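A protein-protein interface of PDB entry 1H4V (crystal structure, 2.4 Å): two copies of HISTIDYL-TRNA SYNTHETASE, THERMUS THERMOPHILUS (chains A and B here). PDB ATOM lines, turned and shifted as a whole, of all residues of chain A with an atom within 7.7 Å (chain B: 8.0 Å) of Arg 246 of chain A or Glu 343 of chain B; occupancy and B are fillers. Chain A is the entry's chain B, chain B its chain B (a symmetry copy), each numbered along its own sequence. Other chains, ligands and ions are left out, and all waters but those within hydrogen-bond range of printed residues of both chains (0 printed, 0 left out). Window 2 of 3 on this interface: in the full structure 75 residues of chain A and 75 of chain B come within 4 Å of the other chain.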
ATOM      1  N   ILE A 138     -18.056  10.377 -19.302  1.00  0.00           N
ATOM      2  CA  ILE A 138     -18.779  11.629 -19.408  1.00  0.00           C
ATOM      3  C   ILE A 138     -18.658  12.362 -18.064  1.00  0.00           C
ATOM      4  O   ILE A 138     -18.519  13.577 -18.026  1.00  0.00           O
ATOM      5  CB  ILE A 138     -20.277  11.385 -19.760  1.00  0.00           C
ATOM      6  CG1 ILE A 138     -20.410  11.118 -21.263  1.00  0.00           C
ATOM      7  CG2 ILE A 138     -21.129  12.579 -19.352  1.00  0.00           C
ATOM      8  CD1 ILE A 138     -21.795  10.650 -21.710  1.00  0.00           C
ATOM      9  N   VAL A 240     -12.548  11.056 -22.518  1.00  0.00           N
ATOM     10  CA  VAL A 240     -12.563  12.298 -21.760  1.00  0.00           C
ATOM     11  C   VAL A 240     -12.068  13.454 -22.630  1.00  0.00           C
ATOM     12  O   VAL A 240     -12.659  14.539 -22.636  1.00  0.00           O
ATOM     13  CB  VAL A 240     -11.675  12.211 -20.500  1.00  0.00           C
ATOM     14  CG1 VAL A 240     -11.755  13.515 -19.715  1.00  0.00           C
ATOM     15  CG2 VAL A 240     -12.113  11.045 -19.635  1.00  0.00           C
ATOM     16  N   GLU A 241     -10.983  13.215 -23.364  1.00  0.00           N
ATOM     17  CA  GLU A 241     -10.420  14.236 -24.240  1.00  0.00           C
ATOM     18  C   GLU A 241     -11.439  14.646 -25.299  1.00  0.00           C
ATOM     19  O   GLU A 241     -11.619  15.834 -25.573  1.00  0.00           O
ATOM     20  CB  GLU A 241      -9.161  13.719 -24.936  1.00  0.00           C
ATOM     21  CG  GLU A 241      -8.003  13.401 -24.009  1.00  0.00           C
ATOM     22  CD  GLU A 241      -6.787  12.873 -24.755  1.00  0.00           C
ATOM     23  OE1 GLU A 241      -6.266  13.597 -25.628  1.00  0.00           O
ATOM     24  OE2 GLU A 241      -6.352  11.736 -24.472  1.00  0.00           O
ATOM     25  N   ARG A 242     -12.110  13.664 -25.888  1.00  0.00           N
ATOM     26  CA  ARG A 242     -13.095  13.949 -26.920  1.00  0.00           C
ATOM     27  C   ARG A 242     -14.185  14.882 -26.403  1.00  0.00           C
ATOM     28  O   ARG A 242     -14.556  15.843 -27.081  1.00  0.00           O
ATOM     29  CB  ARG A 242     -13.724  12.653 -27.443  1.00  0.00           C
ATOM     30  CG  ARG A 242     -14.617  12.878 -28.656  1.00  0.00           C
ATOM     31  CD  ARG A 242     -15.244  11.584 -29.158  1.00  0.00           C
ATOM     32  NE  ARG A 242     -16.307  11.109 -28.274  1.00  0.00           N
ATOM     33  CZ  ARG A 242     -17.058  10.039 -28.521  1.00  0.00           C
ATOM     34  NH1 ARG A 242     -16.857   9.332 -29.625  1.00  0.00           N
ATOM     35  NH2 ARG A 242     -18.016   9.685 -27.673  1.00  0.00           N
ATOM     36  N   HIS A 243     -14.690  14.613 -25.200  1.00  0.00           N
ATOM     37  CA  HIS A 243     -15.728  15.464 -24.635  1.00  0.00           C
ATOM     38  C   HIS A 243     -15.284  16.906 -24.415  1.00  0.00           C
ATOM     39  O   HIS A 243     -16.029  17.832 -24.734  1.00  0.00           O
ATOM     40  CB  HIS A 243     -16.257  14.875 -23.325  1.00  0.00           C
ATOM     41  CG  HIS A 243     -16.919  13.546 -23.496  1.00  0.00           C
ATOM     42  ND1 HIS A 243     -17.752  13.263 -24.558  1.00  0.00           N
ATOM     43  CD2 HIS A 243     -16.859  12.417 -22.752  1.00  0.00           C
ATOM     44  CE1 HIS A 243     -18.173  12.015 -24.464  1.00  0.00           C
ATOM     45  NE2 HIS A 243     -17.646  11.479 -23.378  1.00  0.00           N
ATOM     46  N   LEU A 244     -14.078  17.109 -23.885  1.00  0.00           N
ATOM     47  CA  LEU A 244     -13.592  18.468 -23.647  1.00  0.00           C
ATOM     48  C   LEU A 244     -13.433  19.234 -24.955  1.00  0.00           C
ATOM     49  O   LEU A 244     -13.750  20.424 -25.034  1.00  0.00           O
ATOM     50  CB  LEU A 244     -12.262  18.445 -22.893  1.00  0.00           C
ATOM     51  CG  LEU A 244     -12.303  17.856 -21.476  1.00  0.00           C
ATOM     52  CD1 LEU A 244     -10.904  17.869 -20.888  1.00  0.00           C
ATOM     53  CD2 LEU A 244     -13.272  18.654 -20.608  1.00  0.00           C
ATOM     54  N   GLU A 245     -12.935  18.555 -25.981  1.00  0.00           N
ATOM     55  CA  GLU A 245     -12.769  19.186 -27.281  1.00  0.00           C
ATOM     56  C   GLU A 245     -14.147  19.664 -27.736  1.00  0.00           C
ATOM     57  O   GLU A 245     -14.326  20.819 -28.122  1.00  0.00           O
ATOM     58  CB  GLU A 245     -12.180  18.175 -28.279  1.00  0.00           C
ATOM     59  N   ARG A 246     -15.121  18.765 -27.650  1.00  0.00           N
ATOM     60  CA  ARG A 246     -16.489  19.046 -28.044  1.00  0.00           C
ATOM     61  C   ARG A 246     -17.126  20.163 -27.202  1.00  0.00           C
ATOM     62  O   ARG A 246     -18.077  20.807 -27.634  1.00  0.00           O
ATOM     63  CB  ARG A 246     -17.299  17.754 -27.938  1.00  0.00           C
ATOM     64  CG  ARG A 246     -18.702  17.847 -28.475  1.00  0.00           C
ATOM     65  CD  ARG A 246     -18.741  18.073 -29.980  1.00  0.00           C
ATOM     66  NE  ARG A 246     -20.115  18.301 -30.407  1.00  0.00           N
ATOM     67  CZ  ARG A 246     -21.027  17.342 -30.532  1.00  0.00           C
ATOM     68  NH1 ARG A 246     -20.708  16.082 -30.280  1.00  0.00           N
ATOM     69  NH2 ARG A 246     -22.273  17.654 -30.859  1.00  0.00           N
ATOM     70  N   LEU A 247     -16.598  20.393 -26.005  1.00  0.00           N
ATOM     71  CA  LEU A 247     -17.126  21.439 -25.134  1.00  0.00           C
ATOM     72  C   LEU A 247     -16.278  22.701 -25.191  1.00  0.00           C
ATOM     73  O   LEU A 247     -16.457  23.618 -24.394  1.00  0.00           O
ATOM     74  CB  LEU A 247     -17.194  20.936 -23.697  1.00  0.00           C
ATOM     75  CG  LEU A 247     -18.325  19.939 -23.444  1.00  0.00           C
ATOM     76  CD1 LEU A 247     -18.075  19.163 -22.163  1.00  0.00           C
ATOM     77  CD2 LEU A 247     -19.638  20.692 -23.396  1.00  0.00           C
ATOM     78  N   SER A 248     -15.356  22.741 -26.144  1.00  0.00           N
ATOM     79  CA  SER A 248     -14.473  23.884 -26.313  1.00  0.00           C
ATOM     80  C   SER A 248     -13.652  24.228 -25.076  1.00  0.00           C
ATOM     81  O   SER A 248     -13.287  25.387 -24.876  1.00  0.00           O
ATOM     82  CB  SER A 248     -15.266  25.119 -26.761  1.00  0.00           C
ATOM     83  OG  SER A 248     -15.568  25.056 -28.145  1.00  0.00           O
ATOM     84  N   VAL A 249     -13.354  23.236 -24.244  1.00  0.00           N
ATOM     85  CA  VAL A 249     -12.534  23.496 -23.065  1.00  0.00           C
ATOM     86  C   VAL A 249     -11.072  23.264 -23.430  1.00  0.00           C
ATOM     87  O   VAL A 249     -10.653  22.136 -23.689  1.00  0.00           O
ATOM     88  CB  VAL A 249     -12.909  22.574 -21.866  1.00  0.00           C
ATOM     89  CG1 VAL A 249     -11.832  22.643 -20.790  1.00  0.00           C
ATOM     90  CG2 VAL A 249     -14.242  23.009 -21.273  1.00  0.00           C
ATOM     91  N   TYR A 251      -7.402  22.396 -23.084  1.00  0.00           N
ATOM     92  CA  TYR A 251      -6.631  21.633 -22.116  1.00  0.00           C
ATOM     93  C   TYR A 251      -5.287  21.220 -22.698  1.00  0.00           C
ATOM     94  O   TYR A 251      -5.062  21.296 -23.906  1.00  0.00           O
ATOM     95  CB  TYR A 251      -7.385  20.378 -21.665  1.00  0.00           C
ATOM     96  CG  TYR A 251      -7.412  19.273 -22.691  1.00  0.00           C
ATOM     97  CD1 TYR A 251      -8.293  19.323 -23.770  1.00  0.00           C
ATOM     98  CD2 TYR A 251      -6.539  18.187 -22.598  1.00  0.00           C
ATOM     99  CE1 TYR A 251      -8.306  18.316 -24.734  1.00  0.00           C
ATOM    100  CE2 TYR A 251      -6.541  17.175 -23.559  1.00  0.00           C
ATOM    101  CZ  TYR A 251      -7.430  17.247 -24.626  1.00  0.00           C
ATOM    102  OH  TYR A 251      -7.454  16.256 -25.584  1.00  0.00           O
ATOM    103  N   LEU B 333     -33.045  16.045 -19.753  1.00  0.00           N
ATOM    104  CA  LEU B 333     -32.813  15.446 -21.067  1.00  0.00           C
ATOM    105  C   LEU B 333     -32.760  13.929 -21.082  1.00  0.00           C
ATOM    106  O   LEU B 333     -32.028  13.311 -20.311  1.00  0.00           O
ATOM    107  CB  LEU B 333     -31.512  15.986 -21.651  1.00  0.00           C
ATOM    108  CG  LEU B 333     -31.624  17.368 -22.283  1.00  0.00           C
ATOM    109  CD1 LEU B 333     -30.260  18.038 -22.343  1.00  0.00           C
ATOM    110  CD2 LEU B 333     -32.236  17.218 -23.671  1.00  0.00           C
ATOM    111  N   PRO B 335     -31.772  10.818 -23.387  1.00  0.00           N
ATOM    112  CA  PRO B 335     -31.130  10.357 -24.626  1.00  0.00           C
ATOM    113  C   PRO B 335     -31.824   9.056 -25.024  1.00  0.00           C
ATOM    114  O   PRO B 335     -32.094   8.216 -24.173  1.00  0.00           O
ATOM    115  CB  PRO B 335     -29.671  10.146 -24.210  1.00  0.00           C
ATOM    116  CG  PRO B 335     -29.780   9.770 -22.767  1.00  0.00           C
ATOM    117  CD  PRO B 335     -30.866  10.682 -22.232  1.00  0.00           C
ATOM    118  N   THR B 337     -30.705   7.067 -27.737  1.00  0.00           N
ATOM    119  CA  THR B 337     -29.695   6.129 -28.206  1.00  0.00           C
ATOM    120  C   THR B 337     -28.451   6.353 -27.363  1.00  0.00           C
ATOM    121  O   THR B 337     -28.365   7.335 -26.621  1.00  0.00           O
ATOM    122  CB  THR B 337     -29.324   6.343 -29.698  1.00  0.00           C
ATOM    123  OG1 THR B 337     -28.753   7.646 -29.874  1.00  0.00           O
ATOM    124  CG2 THR B 337     -30.552   6.197 -30.578  1.00  0.00           C
ATOM    125  N   GLU B 338     -27.488   5.447 -27.490  1.00  0.00           N
ATOM    126  CA  GLU B 338     -26.250   5.533 -26.741  1.00  0.00           C
ATOM    127  C   GLU B 338     -25.420   6.730 -27.184  1.00  0.00           C
ATOM    128  O   GLU B 338     -24.742   7.351 -26.372  1.00  0.00           O
ATOM    129  CB  GLU B 338     -25.442   4.250 -26.921  1.00  0.00           C
ATOM    130  CG  GLU B 338     -24.305   4.118 -25.925  1.00  0.00           C
ATOM    131  CD  GLU B 338     -24.793   3.796 -24.518  1.00  0.00           C
ATOM    132  OE1 GLU B 338     -24.032   4.049 -23.557  1.00  0.00           O
ATOM    133  OE2 GLU B 338     -25.925   3.281 -24.371  1.00  0.00           O
ATOM    134  N   GLU B 339     -25.463   7.052 -28.472  1.00  0.00           N
ATOM    135  CA  GLU B 339     -24.701   8.190 -28.987  1.00  0.00           C
ATOM    136  C   GLU B 339     -25.303   9.506 -28.499  1.00  0.00           C
ATOM    137  O   GLU B 339     -24.602  10.513 -28.388  1.00  0.00           O
ATOM    138  CB  GLU B 339     -24.679   8.197 -30.523  1.00  0.00           C
ATOM    139  CG  GLU B 339     -23.981   9.423 -31.117  1.00  0.00           C
ATOM    140  CD  GLU B 339     -24.287   9.650 -32.598  1.00  0.00           C
ATOM    141  OE1 GLU B 339     -23.923  10.735 -33.109  1.00  0.00           O
ATOM    142  OE2 GLU B 339     -24.886   8.759 -33.252  1.00  0.00           O
ATOM    143  N   ALA B 340     -26.598   9.486 -28.199  1.00  0.00           N
ATOM    144  CA  ALA B 340     -27.296  10.677 -27.743  1.00  0.00           C
ATOM    145  C   ALA B 340     -26.966  11.049 -26.290  1.00  0.00           C
ATOM    146  O   ALA B 340     -27.207  12.178 -25.865  1.00  0.00           O
ATOM    147  CB  ALA B 340     -28.794  10.483 -27.913  1.00  0.00           C
ATOM    148  N   VAL B 341     -26.418  10.101 -25.537  1.00  0.00           N
ATOM    149  CA  VAL B 341     -26.044  10.336 -24.142  1.00  0.00           C
ATOM    150  C   VAL B 341     -25.043  11.494 -24.078  1.00  0.00           C
ATOM    151  O   VAL B 341     -25.203  12.432 -23.305  1.00  0.00           O
ATOM    152  CB  VAL B 341     -25.396   9.081 -23.532  1.00  0.00           C
ATOM    153  CG1 VAL B 341     -24.874   9.386 -22.135  1.00  0.00           C
ATOM    154  CG2 VAL B 341     -26.391   7.942 -23.504  1.00  0.00           C
ATOM    155  N   ALA B 342     -24.017  11.428 -24.917  1.00  0.00           N
ATOM    156  CA  ALA B 342     -23.006  12.477 -24.968  1.00  0.00           C
ATOM    157  C   ALA B 342     -23.620  13.792 -25.440  1.00  0.00           C
ATOM    158  O   ALA B 342     -23.308  14.859 -24.911  1.00  0.00           O
ATOM    159  CB  ALA B 342     -21.887  12.072 -25.903  1.00  0.00           C
ATOM    160  N   GLU B 343     -24.487  13.711 -26.442  1.00  0.00           N
ATOM    161  CA  GLU B 343     -25.133  14.900 -26.974  1.00  0.00           C
ATOM    162  C   GLU B 343     -26.029  15.546 -25.914  1.00  0.00           C
ATOM    163  O   GLU B 343     -26.188  16.763 -25.890  1.00  0.00           O
ATOM    164  CB  GLU B 343     -25.961  14.547 -28.213  1.00  0.00           C
ATOM    165  CG  GLU B 343     -25.186  13.855 -29.317  1.00  0.00           C
ATOM    166  CD  GLU B 343     -24.042  14.691 -29.873  1.00  0.00           C
ATOM    167  OE1 GLU B 343     -24.207  15.926 -30.015  1.00  0.00           O
ATOM    168  OE2 GLU B 343     -22.980  14.101 -30.188  1.00  0.00           O
ATOM    169  N   ALA B 344     -26.617  14.735 -25.040  1.00  0.00           N
ATOM    170  CA  ALA B 344     -27.477  15.272 -23.988  1.00  0.00           C
ATOM    171  C   ALA B 344     -26.620  16.083 -23.018  1.00  0.00           C
ATOM    172  O   ALA B 344     -27.041  17.129 -22.501  1.00  0.00           O
ATOM    173  CB  ALA B 344     -28.175  14.144 -23.249  1.00  0.00           C
ATOM    174  N   PHE B 345     -25.411  15.588 -22.783  1.00  0.00           N
ATOM    175  CA  PHE B 345     -24.461  16.235 -21.899  1.00  0.00           C
ATOM    176  C   PHE B 345     -24.016  17.554 -22.516  1.00  0.00           C
ATOM    177  O   PHE B 345     -23.980  18.572 -21.836  1.00  0.00           O
ATOM    178  CB  PHE B 345     -23.269  15.296 -21.669  1.00  0.00           C
ATOM    179  CG  PHE B 345     -22.048  15.967 -21.096  1.00  0.00           C
ATOM    180  CD1 PHE B 345     -22.120  16.710 -19.916  1.00  0.00           C
ATOM    181  CD2 PHE B 345     -20.808  15.802 -21.705  1.00  0.00           C
ATOM    182  CE1 PHE B 345     -20.974  17.271 -19.349  1.00  0.00           C
ATOM    183  CE2 PHE B 345     -19.650  16.362 -21.141  1.00  0.00           C
ATOM    184  CZ  PHE B 345     -19.734  17.094 -19.963  1.00  0.00           C
ATOM    185  N   TYR B 346     -23.707  17.544 -23.809  1.00  0.00           N
ATOM    186  CA  TYR B 346     -23.254  18.763 -24.495  1.00  0.00           C
ATOM    187  C   TYR B 346     -24.327  19.832 -24.479  1.00  0.00           C
ATOM    188  O   TYR B 346     -24.029  21.009 -24.300  1.00  0.00           O
ATOM    189  CB  TYR B 346     -22.882  18.466 -25.944  1.00  0.00           C
ATOM    190  CG  TYR B 346     -21.807  17.420 -26.090  1.00  0.00           C
ATOM    191  CD1 TYR B 346     -21.742  16.619 -27.225  1.00  0.00           C
ATOM    192  CD2 TYR B 346     -20.855  17.225 -25.092  1.00  0.00           C
ATOM    193  CE1 TYR B 346     -20.760  15.649 -27.361  1.00  0.00           C
ATOM    194  CE2 TYR B 346     -19.867  16.260 -25.221  1.00  0.00           C
ATOM    195  CZ  TYR B 346     -19.825  15.474 -26.359  1.00  0.00           C
ATOM    196  OH  TYR B 346     -18.846  14.511 -26.499  1.00  0.00           O
ATOM    197  N   LEU B 347     -25.576  19.419 -24.673  1.00  0.00           N
ATOM    198  CA  LEU B 347     -26.692  20.354 -24.676  1.00  0.00           C
ATOM    199  C   LEU B 347     -26.923  20.919 -23.274  1.00  0.00           C
ATOM    200  O   LEU B 347     -27.074  22.124 -23.108  1.00  0.00           O
ATOM    201  CB  LEU B 347     -27.969  19.666 -25.184  1.00  0.00           C
ATOM    202  CG  LEU B 347     -29.249  20.507 -25.101  1.00  0.00           C
ATOM    203  CD1 LEU B 347     -29.054  21.820 -25.838  1.00  0.00           C
ATOM    204  CD2 LEU B 347     -30.419  19.719 -25.699  1.00  0.00           C
ATOM    205  N   ALA B 348     -26.954  20.051 -22.266  1.00  0.00           N
ATOM    206  CA  ALA B 348     -27.155  20.515 -20.897  1.00  0.00           C
ATOM    207  C   ALA B 348     -26.038  21.499 -20.504  1.00  0.00           C
ATOM    208  O   ALA B 348     -26.299  22.529 -19.881  1.00  0.00           O
ATOM    209  CB  ALA B 348     -27.182  19.330 -19.936  1.00  0.00           C
ATOM    210  N   GLU B 349     -24.800  21.189 -20.870  1.00  0.00           N
ATOM    211  CA  GLU B 349     -23.695  22.078 -20.543  1.00  0.00           C
ATOM    212  C   GLU B 349     -23.838  23.438 -21.225  1.00  0.00           C
ATOM    213  O   GLU B 349     -23.410  24.455 -20.687  1.00  0.00           O
ATOM    214  CB  GLU B 349     -22.356  21.445 -20.922  1.00  0.00           C
ATOM    215  CG  GLU B 349     -21.559  20.933 -19.724  1.00  0.00           C
ATOM    216  CD  GLU B 349     -21.272  22.029 -18.702  1.00  0.00           C
ATOM    217  OE1 GLU B 349     -20.697  23.073 -19.090  1.00  0.00           O
ATOM    218  OE2 GLU B 349     -21.620  21.851 -17.509  1.00  0.00           O
ATOM    219  N   ALA B 350     -24.457  23.453 -22.402  1.00  0.00           N
ATOM    220  CA  ALA B 350     -24.661  24.692 -23.146  1.00  0.00           C
ATOM    221  C   ALA B 350     -25.742  25.557 -22.505  1.00  0.00           C
ATOM    222  O   ALA B 350     -25.812  26.761 -22.749  1.00  0.00           O
ATOM    223  CB  ALA B 350     -25.049  24.373 -24.594  1.00  0.00           C
ATOM    224  N   TYR B 359     -29.512  15.345 -17.193  1.00  0.00           N
ATOM    225  CA  TYR B 359     -29.688  14.337 -18.222  1.00  0.00           C
ATOM    226  C   TYR B 359     -29.444  12.938 -17.677  1.00  0.00           C
ATOM    227  O   TYR B 359     -28.715  12.763 -16.707  1.00  0.00           O
ATOM    228  CB  TYR B 359     -28.707  14.624 -19.360  1.00  0.00           C
ATOM    229  CG  TYR B 359     -27.268  14.625 -18.895  1.00  0.00           C
ATOM    230  CD1 TYR B 359     -26.565  13.428 -18.733  1.00  0.00           C
ATOM    231  CD2 TYR B 359     -26.632  15.813 -18.534  1.00  0.00           C
ATOM    232  CE1 TYR B 359     -25.275  13.415 -18.215  1.00  0.00           C
ATOM    233  CE2 TYR B 359     -25.340  15.810 -18.017  1.00  0.00           C
ATOM    234  CZ  TYR B 359     -24.672  14.607 -17.856  1.00  0.00           C
ATOM    235  OH  TYR B 359     -23.417  14.592 -17.296  1.00  0.00           O
ATOM    236  N   LEU B 384     -33.610  13.278 -27.098  1.00  0.00           N
ATOM    237  CA  LEU B 384     -32.585  13.246 -28.128  1.00  0.00           C
ATOM    238  C   LEU B 384     -32.430  11.836 -28.688  1.00  0.00           C
ATOM    239  O   LEU B 384     -31.999  10.912 -27.994  1.00  0.00           O
ATOM    240  CB  LEU B 384     -31.246  13.720 -27.569  1.00  0.00           C
ATOM    241  CG  LEU B 384     -31.088  15.193 -27.204  1.00  0.00           C
ATOM    242  CD1 LEU B 384     -29.735  15.384 -26.525  1.00  0.00           C
ATOM    243  CD2 LEU B 384     -31.171  16.055 -28.452  1.00  0.00           C
ATOM    244  N   GLY B 385     -32.799  11.683 -29.949  1.00  0.00           N
ATOM    245  CA  GLY B 385     -32.689  10.399 -30.596  1.00  0.00           C
ATOM    246  C   GLY B 385     -31.988  10.570 -31.924  1.00  0.00           C
ATOM    247  O   GLY B 385     -31.535  11.668 -32.273  1.00  0.00           O
ATOM    248  N   GLU B 388     -33.395  13.593 -34.041  1.00  0.00           N
ATOM    249  CA  GLU B 388     -32.975  14.941 -33.677  1.00  0.00           C
ATOM    250  C   GLU B 388     -31.471  15.122 -33.821  1.00  0.00           C
ATOM    251  O   GLU B 388     -31.006  16.218 -34.139  1.00  0.00           O
ATOM    252  CB  GLU B 388     -33.416  15.334 -32.256  1.00  0.00           C
ATOM    253  CG  GLU B 388     -33.718  14.199 -31.294  1.00  0.00           C
ATOM    254  CD  GLU B 388     -35.087  13.592 -31.521  1.00  0.00           C
ATOM    255  OE1 GLU B 388     -36.067  14.365 -31.562  1.00  0.00           O
ATOM    256  OE2 GLU B 388     -35.179  12.351 -31.651  1.00  0.00           O
ATOM    257  N   LEU B 389     -30.710  14.055 -33.613  1.00  0.00           N
ATOM    258  CA  LEU B 389     -29.263  14.158 -33.749  1.00  0.00           C
ATOM    259  C   LEU B 389     -28.865  14.475 -35.188  1.00  0.00           C
ATOM    260  O   LEU B 389     -28.016  15.327 -35.426  1.00  0.00           O
ATOM    261  CB  LEU B 389     -28.574  12.873 -33.282  1.00  0.00           C
ATOM    262  CG  LEU B 389     -28.537  12.625 -31.764  1.00  0.00           C
ATOM    263  CD1 LEU B 389     -27.604  11.459 -31.460  1.00  0.00           C
ATOM    264  CD2 LEU B 389     -28.049  13.871 -31.043  1.00  0.00           C
ATOM    265  N   GLY B 392     -29.846  17.999 -35.882  1.00  0.00           N
ATOM    266  CA  GLY B 392     -29.276  19.023 -35.021  1.00  0.00           C
ATOM    267  C   GLY B 392     -30.400  19.776 -34.327  1.00  0.00           C
ATOM    268  O   GLY B 392     -30.381  21.002 -34.223  1.00  0.00           O
ATOM    269  N   GLU B 393     -31.389  19.024 -33.855  1.00  0.00           N
ATOM    270  CA  GLU B 393     -32.549  19.589 -33.184  1.00  0.00           C
ATOM    271  C   GLU B 393     -32.809  18.896 -31.854  1.00  0.00           C
ATOM    272  O   GLU B 393     -32.049  18.022 -31.435  1.00  0.00           O
ATOM    273  CB  GLU B 393     -33.786  19.447 -34.077  1.00  0.00           C
ATOM    274  CG  GLU B 393     -33.666  20.175 -35.399  1.00  0.00           C
ATOM    275  CD  GLU B 393     -34.816  19.882 -36.346  1.00  0.00           C
ATOM    276  OE1 GLU B 393     -34.848  20.489 -37.436  1.00  0.00           O
ATOM    277  OE2 GLU B 393     -35.684  19.047 -36.009  1.00  0.00           O
ATOM    278  N   VAL B 394     -33.901  19.288 -31.206  1.00  0.00           N
ATOM    279  CA  VAL B 394     -34.298  18.730 -29.918  1.00  0.00           C
ATOM    280  C   VAL B 394     -35.811  18.773 -29.809  1.00  0.00           C
ATOM    281  O   VAL B 394     -36.469  19.615 -30.431  1.00  0.00           O
ATOM    282  CB  VAL B 394     -33.727  19.558 -28.746  1.00  0.00           C
ATOM    283  CG1 VAL B 394     -33.908  18.811 -27.440  1.00  0.00           C
ATOM    284  CG2 VAL B 394     -32.267  19.867 -28.996  1.00  0.00           C
ATOM    285  N   ARG B 409     -31.021  23.294 -31.832  1.00  0.00           N
ATOM    286  CA  ARG B 409     -30.226  23.509 -30.631  1.00  0.00           C
ATOM    287  C   ARG B 409     -29.912  24.970 -30.336  1.00  0.00           C
ATOM    288  O   ARG B 409     -29.828  25.358 -29.178  1.00  0.00           O
ATOM    289  CB  ARG B 409     -28.925  22.713 -30.699  1.00  0.00           C
ATOM    290  CG  ARG B 409     -29.116  21.229 -30.524  1.00  0.00           C
ATOM    291  CD  ARG B 409     -27.867  20.606 -29.943  1.00  0.00           C
ATOM    292  NE  ARG B 409     -28.015  19.171 -29.722  1.00  0.00           N
ATOM    293  CZ  ARG B 409     -27.160  18.434 -29.022  1.00  0.00           C
ATOM    294  NH1 ARG B 409     -26.092  18.995 -28.466  1.00  0.00           N
ATOM    295  NH2 ARG B 409     -27.369  17.131 -28.886  1.00  0.00           N
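The side-chain hydroxyl (OH) of Tyr 346 of chain B sits at hydrogen-bond distance from a ring nitrogen (ND1) of His 243 of chain A (2.6 Å). The guanidinium group (NH2) of Arg 246 of chain A lies within salt-bridge range of the side-chain carboxylate (OE1) of Glu 343 of chain B (2.7 Å).
OE1 of Glu 343 of chain B is in salt-bridge range of NH2 of Arg 409 of chain B (3.6 Å).
Among the printed residues, merely in contact across the chains: Arg 246 of chain A with Tyr 346 of chain B, Ile 138 of chain A with Val 341 of chain B, Leu 247 of chain A with Phe 345 of chain B, Ile 138 of chain A with Tyr 359 of chain B, Leu 247 of chain A with Glu 349 of chain B, Ile 138 of chain A with Phe 345 of chain B, Ile 138 of chain A with Ala 342 of chain B and His 243 of chain A with Ala 342 of chain B.
Arg 246 of chain A touches just these residues of chain B: Glu 343 and Tyr 346. Of chain A, only Arg 246 comes within 4 Å of Glu 343 of chain B. Of the printed residues of chain A, Ala 342 of chain B touches Ile 138 (3.9 Å) and His 243 (3.98 Å). Printed residues of chain A within 4 Å of Glu 349 of chain B: Leu 247 (3.8 Å). Printed residues of chain A within 4 Å of Tyr 346 of chain B: His 243 and Arg 246. Printed residues of chain A within 4 Å of Phe 345 of chain B: Ile 138 and Leu 247. The nearest printed residue of chain A that does not touch Ala 342 of chain B is Arg 242 of chain A (4.9 Å).
Printed residues of chain A that touch a printed residue of chain B: Ile 138, His 243, Arg 246 and Leu 247. Along chain A the printed residues that touch a printed residue of chain B span positions 138 to 247. Among the printed residues, Asp or Glu carboxylates within 4 Å of a Lys or Arg side-chain nitrogen of the other chain: Arg 246 of chain A with Glu 343 of chain B.
No position is printed for both chains.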
